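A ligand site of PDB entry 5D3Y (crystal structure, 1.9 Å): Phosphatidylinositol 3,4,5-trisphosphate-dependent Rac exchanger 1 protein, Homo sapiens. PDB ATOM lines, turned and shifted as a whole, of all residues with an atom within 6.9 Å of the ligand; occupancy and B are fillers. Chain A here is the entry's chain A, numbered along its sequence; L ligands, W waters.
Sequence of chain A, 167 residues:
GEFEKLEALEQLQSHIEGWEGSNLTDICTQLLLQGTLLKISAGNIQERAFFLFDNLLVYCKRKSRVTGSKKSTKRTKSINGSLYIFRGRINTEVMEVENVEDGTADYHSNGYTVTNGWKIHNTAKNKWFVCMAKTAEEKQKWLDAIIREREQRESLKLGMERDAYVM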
ATOM      1  N   LYS A  39       1.245  10.909  -0.145  1.00  0.00           N
ATOM      2  CA  LYS A  39       0.064  10.385   0.544  1.00  0.00           C
ATOM      3  C   LYS A  39       0.504   9.614   1.789  1.00  0.00           C
ATOM      4  O   LYS A  39       1.262   8.677   1.680  1.00  0.00           O
ATOM      5  CB  LYS A  39      -0.776   9.475  -0.384  1.00  0.00           C
ATOM      6  CG  LYS A  39      -1.931   8.853   0.362  1.00  0.00           C
ATOM      7  CD  LYS A  39      -3.016   8.250  -0.533  1.00  0.00           C
ATOM      8  CE  LYS A  39      -2.628   6.960  -1.176  1.00  0.00           C
ATOM      9  NZ  LYS A  39      -2.319   5.825  -0.240  1.00  0.00           N
ATOM     10  N   ILE A  40       0.030  10.018   2.975  1.00  0.00           N
ATOM     11  CA  ILE A  40       0.238   9.219   4.201  1.00  0.00           C
ATOM     12  C   ILE A  40      -1.039   8.374   4.432  1.00  0.00           C
ATOM     13  O   ILE A  40      -2.124   8.914   4.607  1.00  0.00           O
ATOM     14  CB  ILE A  40       0.544  10.115   5.459  1.00  0.00           C
ATOM     15  CG1 ILE A  40       1.664  11.132   5.200  1.00  0.00           C
ATOM     16  CG2 ILE A  40       0.959   9.251   6.648  1.00  0.00           C
ATOM     17  CD1 ILE A  40       1.768  12.178   6.273  1.00  0.00           C
ATOM     18  N   SER A  41      -0.905   7.054   4.394  1.00  0.00           N
ATOM     19  CA  SER A  41      -2.040   6.162   4.606  1.00  0.00           C
ATOM     20  C   SER A  41      -1.624   4.903   5.366  1.00  0.00           C
ATOM     21  O   SER A  41      -0.643   4.264   4.999  1.00  0.00           O
ATOM     22  CB  SER A  41      -2.668   5.796   3.248  1.00  0.00           C
ATOM     23  OG  SER A  41      -3.782   4.915   3.433  1.00  0.00           O
ATOM     24  N   ALA A  42      -2.386   4.543   6.411  1.00  0.00           N
ATOM     25  CA  ALA A  42      -2.093   3.329   7.179  1.00  0.00           C
ATOM     26  C   ALA A  42      -0.637   3.315   7.648  1.00  0.00           C
ATOM     27  O   ALA A  42       0.018   2.280   7.595  1.00  0.00           O
ATOM     28  CB  ALA A  42      -2.373   2.085   6.341  1.00  0.00           C
ATOM     29  N   GLY A  43      -0.111   4.479   8.012  1.00  0.00           N
ATOM     30  CA  GLY A  43       1.283   4.553   8.427  1.00  0.00           C
ATOM     31  C   GLY A  43       2.387   4.628   7.361  1.00  0.00           C
ATOM     32  O   GLY A  43       3.548   4.773   7.717  1.00  0.00           O
ATOM     33  N   ASN A  44       2.031   4.508   6.083  1.00  0.00           N
ATOM     34  CA  ASN A  44       2.987   4.558   4.973  1.00  0.00           C
ATOM     35  C   ASN A  44       3.037   5.908   4.312  1.00  0.00           C
ATOM     36  O   ASN A  44       2.014   6.583   4.232  1.00  0.00           O
ATOM     37  CB  ASN A  44       2.635   3.562   3.860  1.00  0.00           C
ATOM     38  CG  ASN A  44       2.537   2.160   4.356  1.00  0.00           C
ATOM     39  OD1 ASN A  44       3.273   1.756   5.239  1.00  0.00           O
ATOM     40  ND2 ASN A  44       1.600   1.419   3.808  1.00  0.00           N
ATOM     41  N   ILE A  45       4.201   6.287   3.788  1.00  0.00           N
ATOM     42  CA  ILE A  45       4.207   7.476   2.922  1.00  0.00           C
ATOM     43  C   ILE A  45       4.631   7.035   1.533  1.00  0.00           C
ATOM     44  O   ILE A  45       5.649   6.399   1.369  1.00  0.00           O
ATOM     45  CB  ILE A  45       5.157   8.559   3.406  1.00  0.00           C
ATOM     46  CG1 ILE A  45       4.850   8.914   4.845  1.00  0.00           C
ATOM     47  CG2 ILE A  45       5.023   9.802   2.491  1.00  0.00           C
ATOM     48  CD1 ILE A  45       5.721   9.991   5.391  1.00  0.00           C
ATOM     49  N   GLN A  46       3.823   7.389   0.533  1.00  0.00           N
ATOM     50  CA  GLN A  46       4.065   7.008  -0.846  1.00  0.00           C
ATOM     51  C   GLN A  46       3.687   8.198  -1.737  1.00  0.00           C
ATOM     52  O   GLN A  46       2.745   8.900  -1.408  1.00  0.00           O
ATOM     53  CB  GLN A  46       3.233   5.808  -1.204  1.00  0.00           C
ATOM     54  CG  GLN A  46       3.700   4.474  -0.541  1.00  0.00           C
ATOM     55  CD  GLN A  46       2.559   3.514  -0.342  1.00  0.00           C
ATOM     56  OE1 GLN A  46       1.563   3.847   0.311  1.00  0.00           O
ATOM     57  NE2 GLN A  46       2.681   2.317  -0.908  1.00  0.00           N
ATOM     58  N   GLU A  47       4.389   8.401  -2.839  1.00  0.00           N
ATOM     59  CA  GLU A  47       4.019   9.446  -3.796  1.00  0.00           C
ATOM     60  C   GLU A  47       2.986   8.871  -4.764  1.00  0.00           C
ATOM     61  O   GLU A  47       3.131   7.726  -5.254  1.00  0.00           O
ATOM     62  CB  GLU A  47       5.246   9.965  -4.583  1.00  0.00           C
ATOM     63  CG  GLU A  47       4.932  11.283  -5.328  1.00  0.00           C
ATOM     64  CD  GLU A  47       6.104  11.799  -6.110  1.00  0.00           C
ATOM     65  OE1 GLU A  47       5.873  12.249  -7.254  1.00  0.00           O
ATOM     66  OE2 GLU A  47       7.231  11.782  -5.589  1.00  0.00           O
ATOM     67  N   ARG A  48       1.967   9.646  -5.104  1.00  0.00           N
ATOM     68  CA  ARG A  48       0.971   9.149  -6.038  1.00  0.00           C
ATOM     69  C   ARG A  48       0.613  10.276  -6.985  1.00  0.00           C
ATOM     70  O   ARG A  48       0.658  11.449  -6.590  1.00  0.00           O
ATOM     71  CB  ARG A  48      -0.296   8.664  -5.305  1.00  0.00           C
ATOM     72  CG  ARG A  48      -0.083   7.514  -4.389  1.00  0.00           C
ATOM     73  CD  ARG A  48      -0.043   6.264  -5.187  1.00  0.00           C
ATOM     74  NE  ARG A  48       0.189   5.052  -4.399  1.00  0.00           N
ATOM     75  CZ  ARG A  48       1.346   4.430  -4.355  1.00  0.00           C
ATOM     76  NH1 ARG A  48       2.392   4.911  -5.039  1.00  0.00           N
ATOM     77  NH2 ARG A  48       1.453   3.328  -3.662  1.00  0.00           N
ATOM     78  N   TYR A  59      -6.316   8.065  -7.780  1.00  0.00           N
ATOM     79  CA  TYR A  59      -4.866   8.135  -7.596  1.00  0.00           C
ATOM     80  C   TYR A  59      -4.153   6.872  -8.051  1.00  0.00           C
ATOM     81  O   TYR A  59      -4.703   5.755  -7.977  1.00  0.00           O
ATOM     82  CB  TYR A  59      -4.477   8.489  -6.148  1.00  0.00           C
ATOM     83  CG  TYR A  59      -5.112   7.642  -5.104  1.00  0.00           C
ATOM     84  CD1 TYR A  59      -6.369   7.937  -4.615  1.00  0.00           C
ATOM     85  CD2 TYR A  59      -4.423   6.571  -4.563  1.00  0.00           C
ATOM     86  CE1 TYR A  59      -6.950   7.138  -3.617  1.00  0.00           C
ATOM     87  CE2 TYR A  59      -4.994   5.780  -3.583  1.00  0.00           C
ATOM     88  CZ  TYR A  59      -6.244   6.070  -3.110  1.00  0.00           C
ATOM     89  OH  TYR A  59      -6.779   5.289  -2.131  1.00  0.00           O
ATOM     90  N   CYS A  60      -2.959   7.079  -8.583  1.00  0.00           N
ATOM     91  CA  CYS A  60      -2.235   6.064  -9.280  1.00  0.00           C
ATOM     92  C   CYS A  60      -0.810   6.088  -8.823  1.00  0.00           C
ATOM     93  O   CYS A  60      -0.319   7.114  -8.414  1.00  0.00           O
ATOM     94  CB  CYS A  60      -2.254   6.305 -10.797  1.00  0.00           C
ATOM     95  SG  CYS A  60      -3.918   6.271 -11.544  1.00  0.00           S
ATOM     96  N   LYS A  61      -0.162   4.931  -8.890  1.00  0.00           N
ATOM     97  CA  LYS A  61       1.296   4.896  -8.804  1.00  0.00           C
ATOM     98  C   LYS A  61       1.864   5.215 -10.181  1.00  0.00           C
ATOM     99  O   LYS A  61       1.424   4.639 -11.177  1.00  0.00           O
ATOM    100  CB  LYS A  61       1.759   3.531  -8.348  1.00  0.00           C
ATOM    101  CG  LYS A  61       3.278   3.402  -8.323  1.00  0.00           C
ATOM    102  CD  LYS A  61       3.707   1.985  -7.883  1.00  0.00           C
ATOM    103  CE  LYS A  61       5.182   1.754  -8.193  1.00  0.00           C
ATOM    104  NZ  LYS A  61       5.614   0.467  -7.586  1.00  0.00           N
ATOM    105  N   PHE A  86      -3.257   1.980 -11.546  1.00  0.00           N
ATOM    106  CA  PHE A  86      -4.431   2.351 -10.749  1.00  0.00           C
ATOM    107  C   PHE A  86      -4.226   1.928  -9.318  1.00  0.00           C
ATOM    108  O   PHE A  86      -3.859   0.777  -9.076  1.00  0.00           O
ATOM    109  CB  PHE A  86      -5.705   1.696 -11.306  1.00  0.00           C
ATOM    110  CG  PHE A  86      -6.932   1.957 -10.507  1.00  0.00           C
ATOM    111  CD1 PHE A  86      -7.255   1.162  -9.405  1.00  0.00           C
ATOM    112  CD2 PHE A  86      -7.783   2.995 -10.840  1.00  0.00           C
ATOM    113  CE1 PHE A  86      -8.424   1.419  -8.640  1.00  0.00           C
ATOM    114  CE2 PHE A  86      -8.940   3.235 -10.098  1.00  0.00           C
ATOM    115  CZ  PHE A  86      -9.242   2.459  -8.981  1.00  0.00           C
ATOM    116  N   ARG A  87      -4.498   2.817  -8.369  1.00  0.00           N
ATOM    117  CA  ARG A  87      -4.443   2.417  -6.974  1.00  0.00           C
ATOM    118  C   ARG A  87      -5.731   2.726  -6.196  1.00  0.00           C
ATOM    119  O   ARG A  87      -6.108   1.971  -5.306  1.00  0.00           O
ATOM    120  CB  ARG A  87      -3.243   3.065  -6.269  1.00  0.00           C
ATOM    121  CG  ARG A  87      -1.870   2.579  -6.783  1.00  0.00           C
ATOM    122  CD  ARG A  87      -1.606   1.082  -6.552  1.00  0.00           C
ATOM    123  NE  ARG A  87      -2.098   0.659  -5.253  1.00  0.00           N
ATOM    124  CZ  ARG A  87      -2.937  -0.356  -5.062  1.00  0.00           C
ATOM    125  NH1 ARG A  87      -3.367  -1.088  -6.093  1.00  0.00           N
ATOM    126  NH2 ARG A  87      -3.355  -0.648  -3.823  1.00  0.00           N
ATOM    127  N   GLY A  88      -6.437   3.803  -6.537  1.00  0.00           N
ATOM    128  CA  GLY A  88      -7.609   4.155  -5.753  1.00  0.00           C
ATOM    129  C   GLY A  88      -8.581   5.118  -6.423  1.00  0.00           C
ATOM    130  O   GLY A  88      -8.194   5.921  -7.241  1.00  0.00           O
ATOM    131  N   ASN A 122     -12.079   8.707   2.750  1.00  0.00           N
ATOM    132  CA  ASN A 122     -12.552   7.620   1.893  1.00  0.00           C
ATOM    133  C   ASN A 122     -13.553   6.779   2.696  1.00  0.00           C
ATOM    134  O   ASN A 122     -13.182   5.842   3.422  1.00  0.00           O
ATOM    135  CB  ASN A 122     -11.370   6.770   1.397  1.00  0.00           C
ATOM    136  CG  ASN A 122     -11.794   5.696   0.419  1.00  0.00           C
ATOM    137  OD1 ASN A 122     -12.978   5.529   0.107  1.00  0.00           O
ATOM    138  ND2 ASN A 122     -10.818   4.923  -0.056  1.00  0.00           N
ATOM    139  N   LYS A 125     -13.849   2.857   2.490  1.00  0.00           N
ATOM    140  CA  LYS A 125     -12.976   1.996   3.308  1.00  0.00           C
ATOM    141  C   LYS A 125     -12.962   2.446   4.761  1.00  0.00           C
ATOM    142  O   LYS A 125     -12.118   2.011   5.522  1.00  0.00           O
ATOM    143  CB  LYS A 125     -11.528   1.991   2.774  1.00  0.00           C
ATOM    144  CG  LYS A 125     -11.365   1.513   1.344  1.00  0.00           C
ATOM    145  CD  LYS A 125      -9.892   1.615   0.901  1.00  0.00           C
ATOM    146  CE  LYS A 125      -8.976   0.713   1.744  1.00  0.00           C
ATOM    147  NZ  LYS A 125      -7.592   0.656   1.142  1.00  0.00           N
ATOM    148  N   LYS A 127     -11.872   5.176   6.060  1.00  0.00           N
ATOM    149  CA  LYS A 127     -10.569   5.657   6.484  1.00  0.00           C
ATOM    150  C   LYS A 127     -10.274   7.032   5.927  1.00  0.00           C
ATOM    151  O   LYS A 127     -10.898   7.425   4.962  1.00  0.00           O
ATOM    152  CB  LYS A 127      -9.477   4.696   6.035  1.00  0.00           C
ATOM    153  CG  LYS A 127      -9.190   4.758   4.546  1.00  0.00           C
ATOM    154  CD  LYS A 127      -8.157   3.706   4.149  1.00  0.00           C
ATOM    155  CE  LYS A 127      -6.719   4.088   4.505  1.00  0.00           C
ATOM    156  NZ  LYS A 127      -5.759   3.077   3.908  1.00  0.00           N
ATOM    157  N   TRP A 128      -9.352   7.744   6.576  1.00  0.00           N
ATOM    158  CA  TRP A 128      -8.797   8.977   6.080  1.00  0.00           C
ATOM    159  C   TRP A 128      -7.383   8.717   5.546  1.00  0.00           C
ATOM    160  O   TRP A 128      -6.699   7.784   5.999  1.00  0.00           O
ATOM    161  CB  TRP A 128      -8.758  10.033   7.203  1.00  0.00           C
ATOM    162  CG  TRP A 128     -10.130  10.487   7.670  1.00  0.00           C
ATOM    163  CD1 TRP A 128     -10.991   9.806   8.490  1.00  0.00           C
ATOM    164  CD2 TRP A 128     -10.762  11.737   7.373  1.00  0.00           C
ATOM    165  NE1 TRP A 128     -12.117  10.534   8.696  1.00  0.00           N
ATOM    166  CE2 TRP A 128     -12.015  11.718   8.021  1.00  0.00           C
ATOM    167  CE3 TRP A 128     -10.410  12.851   6.600  1.00  0.00           C
ATOM    168  CZ2 TRP A 128     -12.919  12.790   7.928  1.00  0.00           C
ATOM    169  CZ3 TRP A 128     -11.305  13.920   6.506  1.00  0.00           C
ATOM    170  CH2 TRP A 128     -12.555  13.873   7.170  1.00  0.00           C
ATOM    171  N   PHE A 129      -6.919   9.528   4.594  1.00  0.00           N
ATOM    172  CA  PHE A 129      -5.474   9.599   4.372  1.00  0.00           C
ATOM    173  C   PHE A 129      -5.048  11.049   4.215  1.00  0.00           C
ATOM    174  O   PHE A 129      -5.892  11.915   3.994  1.00  0.00           O
ATOM    175  CB  PHE A 129      -5.021   8.793   3.157  1.00  0.00           C
ATOM    176  CG  PHE A 129      -5.725   9.128   1.859  1.00  0.00           C
ATOM    177  CD1 PHE A 129      -5.388  10.265   1.138  1.00  0.00           C
ATOM    178  CD2 PHE A 129      -6.672   8.265   1.335  1.00  0.00           C
ATOM    179  CE1 PHE A 129      -6.030  10.551  -0.066  1.00  0.00           C
ATOM    180  CE2 PHE A 129      -7.319   8.538   0.134  1.00  0.00           C
ATOM    181  CZ  PHE A 129      -6.988   9.680  -0.572  1.00  0.00           C
HETATM  182  C1  LIG L   1      -0.712  -0.125   1.395  1.00  0.00           C
HETATM  183  O1  LIG L   1       0.544  -0.538   1.918  1.00  0.00           O
HETATM  184  C2  LIG L   1      -0.571   1.191   0.646  1.00  0.00           C
HETATM  185  O2  LIG L   1      -0.177   2.183   1.574  1.00  0.00           O
HETATM  186  C3  LIG L   1      -1.888   1.530  -0.060  1.00  0.00           C
HETATM  187  O3  LIG L   1      -1.878   2.825  -0.640  1.00  0.00           O
HETATM  188  C4  LIG L   1      -3.182   1.115   0.671  1.00  0.00           C
HETATM  189  O4  LIG L   1      -4.428   1.826   0.607  1.00  0.00           O
HETATM  190  C5  LIG L   1      -3.091   0.289   1.977  1.00  0.00           C
HETATM  191  O5  LIG L   1      -3.978   0.684   2.992  1.00  0.00           O
HETATM  192  C6  LIG L   1      -1.701   0.034   2.540  1.00  0.00           C
HETATM  193  O6  LIG L   1      -1.817  -1.180   3.266  1.00  0.00           O
HETATM  194  P1  LIG L   1       1.433  -1.387   0.926  1.00  0.00           P
HETATM  195  O7  LIG L   1       2.763  -1.655   1.547  1.00  0.00           O
HETATM  196  O8  LIG L   1       1.738  -0.632  -0.378  1.00  0.00           O
HETATM  197  O9  LIG L   1       0.757  -2.674   0.595  1.00  0.00           O
HETATM  198  P2  LIG L   1      -1.995   2.873  -2.230  1.00  0.00           P
HETATM  199  O10 LIG L   1      -1.839   4.318  -2.677  1.00  0.00           O
HETATM  200  O11 LIG L   1      -3.424   2.436  -2.537  1.00  0.00           O
HETATM  201  O12 LIG L   1      -0.997   2.032  -2.985  1.00  0.00           O
HETATM  202  P3  LIG L   1      -5.045   3.256   0.367  1.00  0.00           P
HETATM  203  O13 LIG L   1      -6.373   3.141   1.049  1.00  0.00           O
HETATM  204  O14 LIG L   1      -5.252   3.502  -1.117  1.00  0.00           O
HETATM  205  O15 LIG L   1      -4.229   4.377   0.999  1.00  0.00           O
HETATM  206  P4  LIG L   1      -5.044  -0.402   3.467  1.00  0.00           P
HETATM  207  O16 LIG L   1      -4.267  -1.553   4.070  1.00  0.00           O
HETATM  208  O17 LIG L   1      -5.923   0.276   4.462  1.00  0.00           O
HETATM  209  O18 LIG L   1      -5.811  -0.953   2.284  1.00  0.00           O
HETATM  210  O   HOH W   1      -7.156   1.938  -2.764  1.00  0.00           O
HETATM  211  O   HOH W   2      -8.074   5.263   0.660  1.00  0.00           O
HETATM  212  O   HOH W   3       0.060  -0.429  -2.730  1.00  0.00           O
HETATM  213  O   HOH W   4       0.099  -0.906   5.488  1.00  0.00           O
HETATM  214  O   HOH W   5      -3.334  -1.886   6.796  1.00  0.00           O
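CB of Ala 42 touches O5 of the ligand, 3.97 Å away.
Hydrophobic or aromatic side chains within 4 Å of the ligand: Ala 42 and Tyr 59.
Ten residues have an atom within 4 Å of the ligand: Lys 39, Ser 41, Ala 42, Asn 44, Gln 46, Arg 48, Tyr 59, Arg 87, Lys 125 and Lys 127.
Water W3 bridges O12 of the ligand (2.7 Å) and NE of Arg 87 (3.5 Å).
Water W2 lies within hydrogen-bond range of O13 of the ligand (2.7 Å), ND2 of Asn 122 (2.9 Å) and OH of Tyr 59 (3.1 Å).
Water W4 bridges an oxygen (O6) of the ligand and the side-chain amide nitrogen of Asn 44.
Water W1 lies within hydrogen-bond range of the backbone carbonyl oxygen (O) of Arg 87 (2.7 Å), an oxygen (O14) of the ligand (3.0 Å) and the side-chain hydroxyl (OH) of Tyr 59 (3.4 Å).
NE of Arg 48 lies within salt-bridge range of O10 of the ligand, at 2.8 Å.
An oxygen (O18) of the ligand lies within salt-bridge range of the side-chain amino group of Lys 125.
The side-chain amino group of Lys 39 is in salt-bridge range of an oxygen (O15) of the ligand, at 2.7 Å.
An oxygen (O17) of the ligand is in salt-bridge range of the side-chain amino group (NZ) of Lys 127.
The side-chain hydroxyl (OH) of Tyr 59 lies within hydrogen-bond range of an oxygen (O14) of the ligand, 2.6 Å away.
The guanidinium group of Arg 87 is in salt-bridge range of an oxygen (O12) of the ligand (2.9 Å).
The side-chain amide oxygen of Gln 46 sits at hydrogen-bond distance from an oxygen (O2) of the ligand (2.7 Å).
The side-chain amide nitrogen (ND2) of Asn 44 is in hydrogen-bond range of an oxygen (O1) of the ligand (2.9 Å).
An oxygen (O15) of the ligand lies within hydrogen-bond range of the side-chain hydroxyl (OG) of Ser 41 (2.5 Å).
The side-chain amino group of Lys 127 is in hydrogen-bond range of the side-chain hydroxyl of Ser 41, 2.7 Å away.
The backbone carbonyl oxygen (O) of Tyr 59 is in hydrogen-bond range of the backbone NH (N) of Arg 87 (3.0 Å).
The backbone NH of Lys 39 sits at hydrogen-bond distance from the backbone carbonyl oxygen of Gln 46 (2.8 Å).
O of Lys 127 sits at hydrogen-bond distance from N of Asn 122 (2.8 Å).
The side-chain amide nitrogen of Gln 46 lies close to the guanidinium group of Arg 48 (3.2 Å).
N of Tyr 59 is in hydrogen-bond range of O of Gly 88 (2.9 Å).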
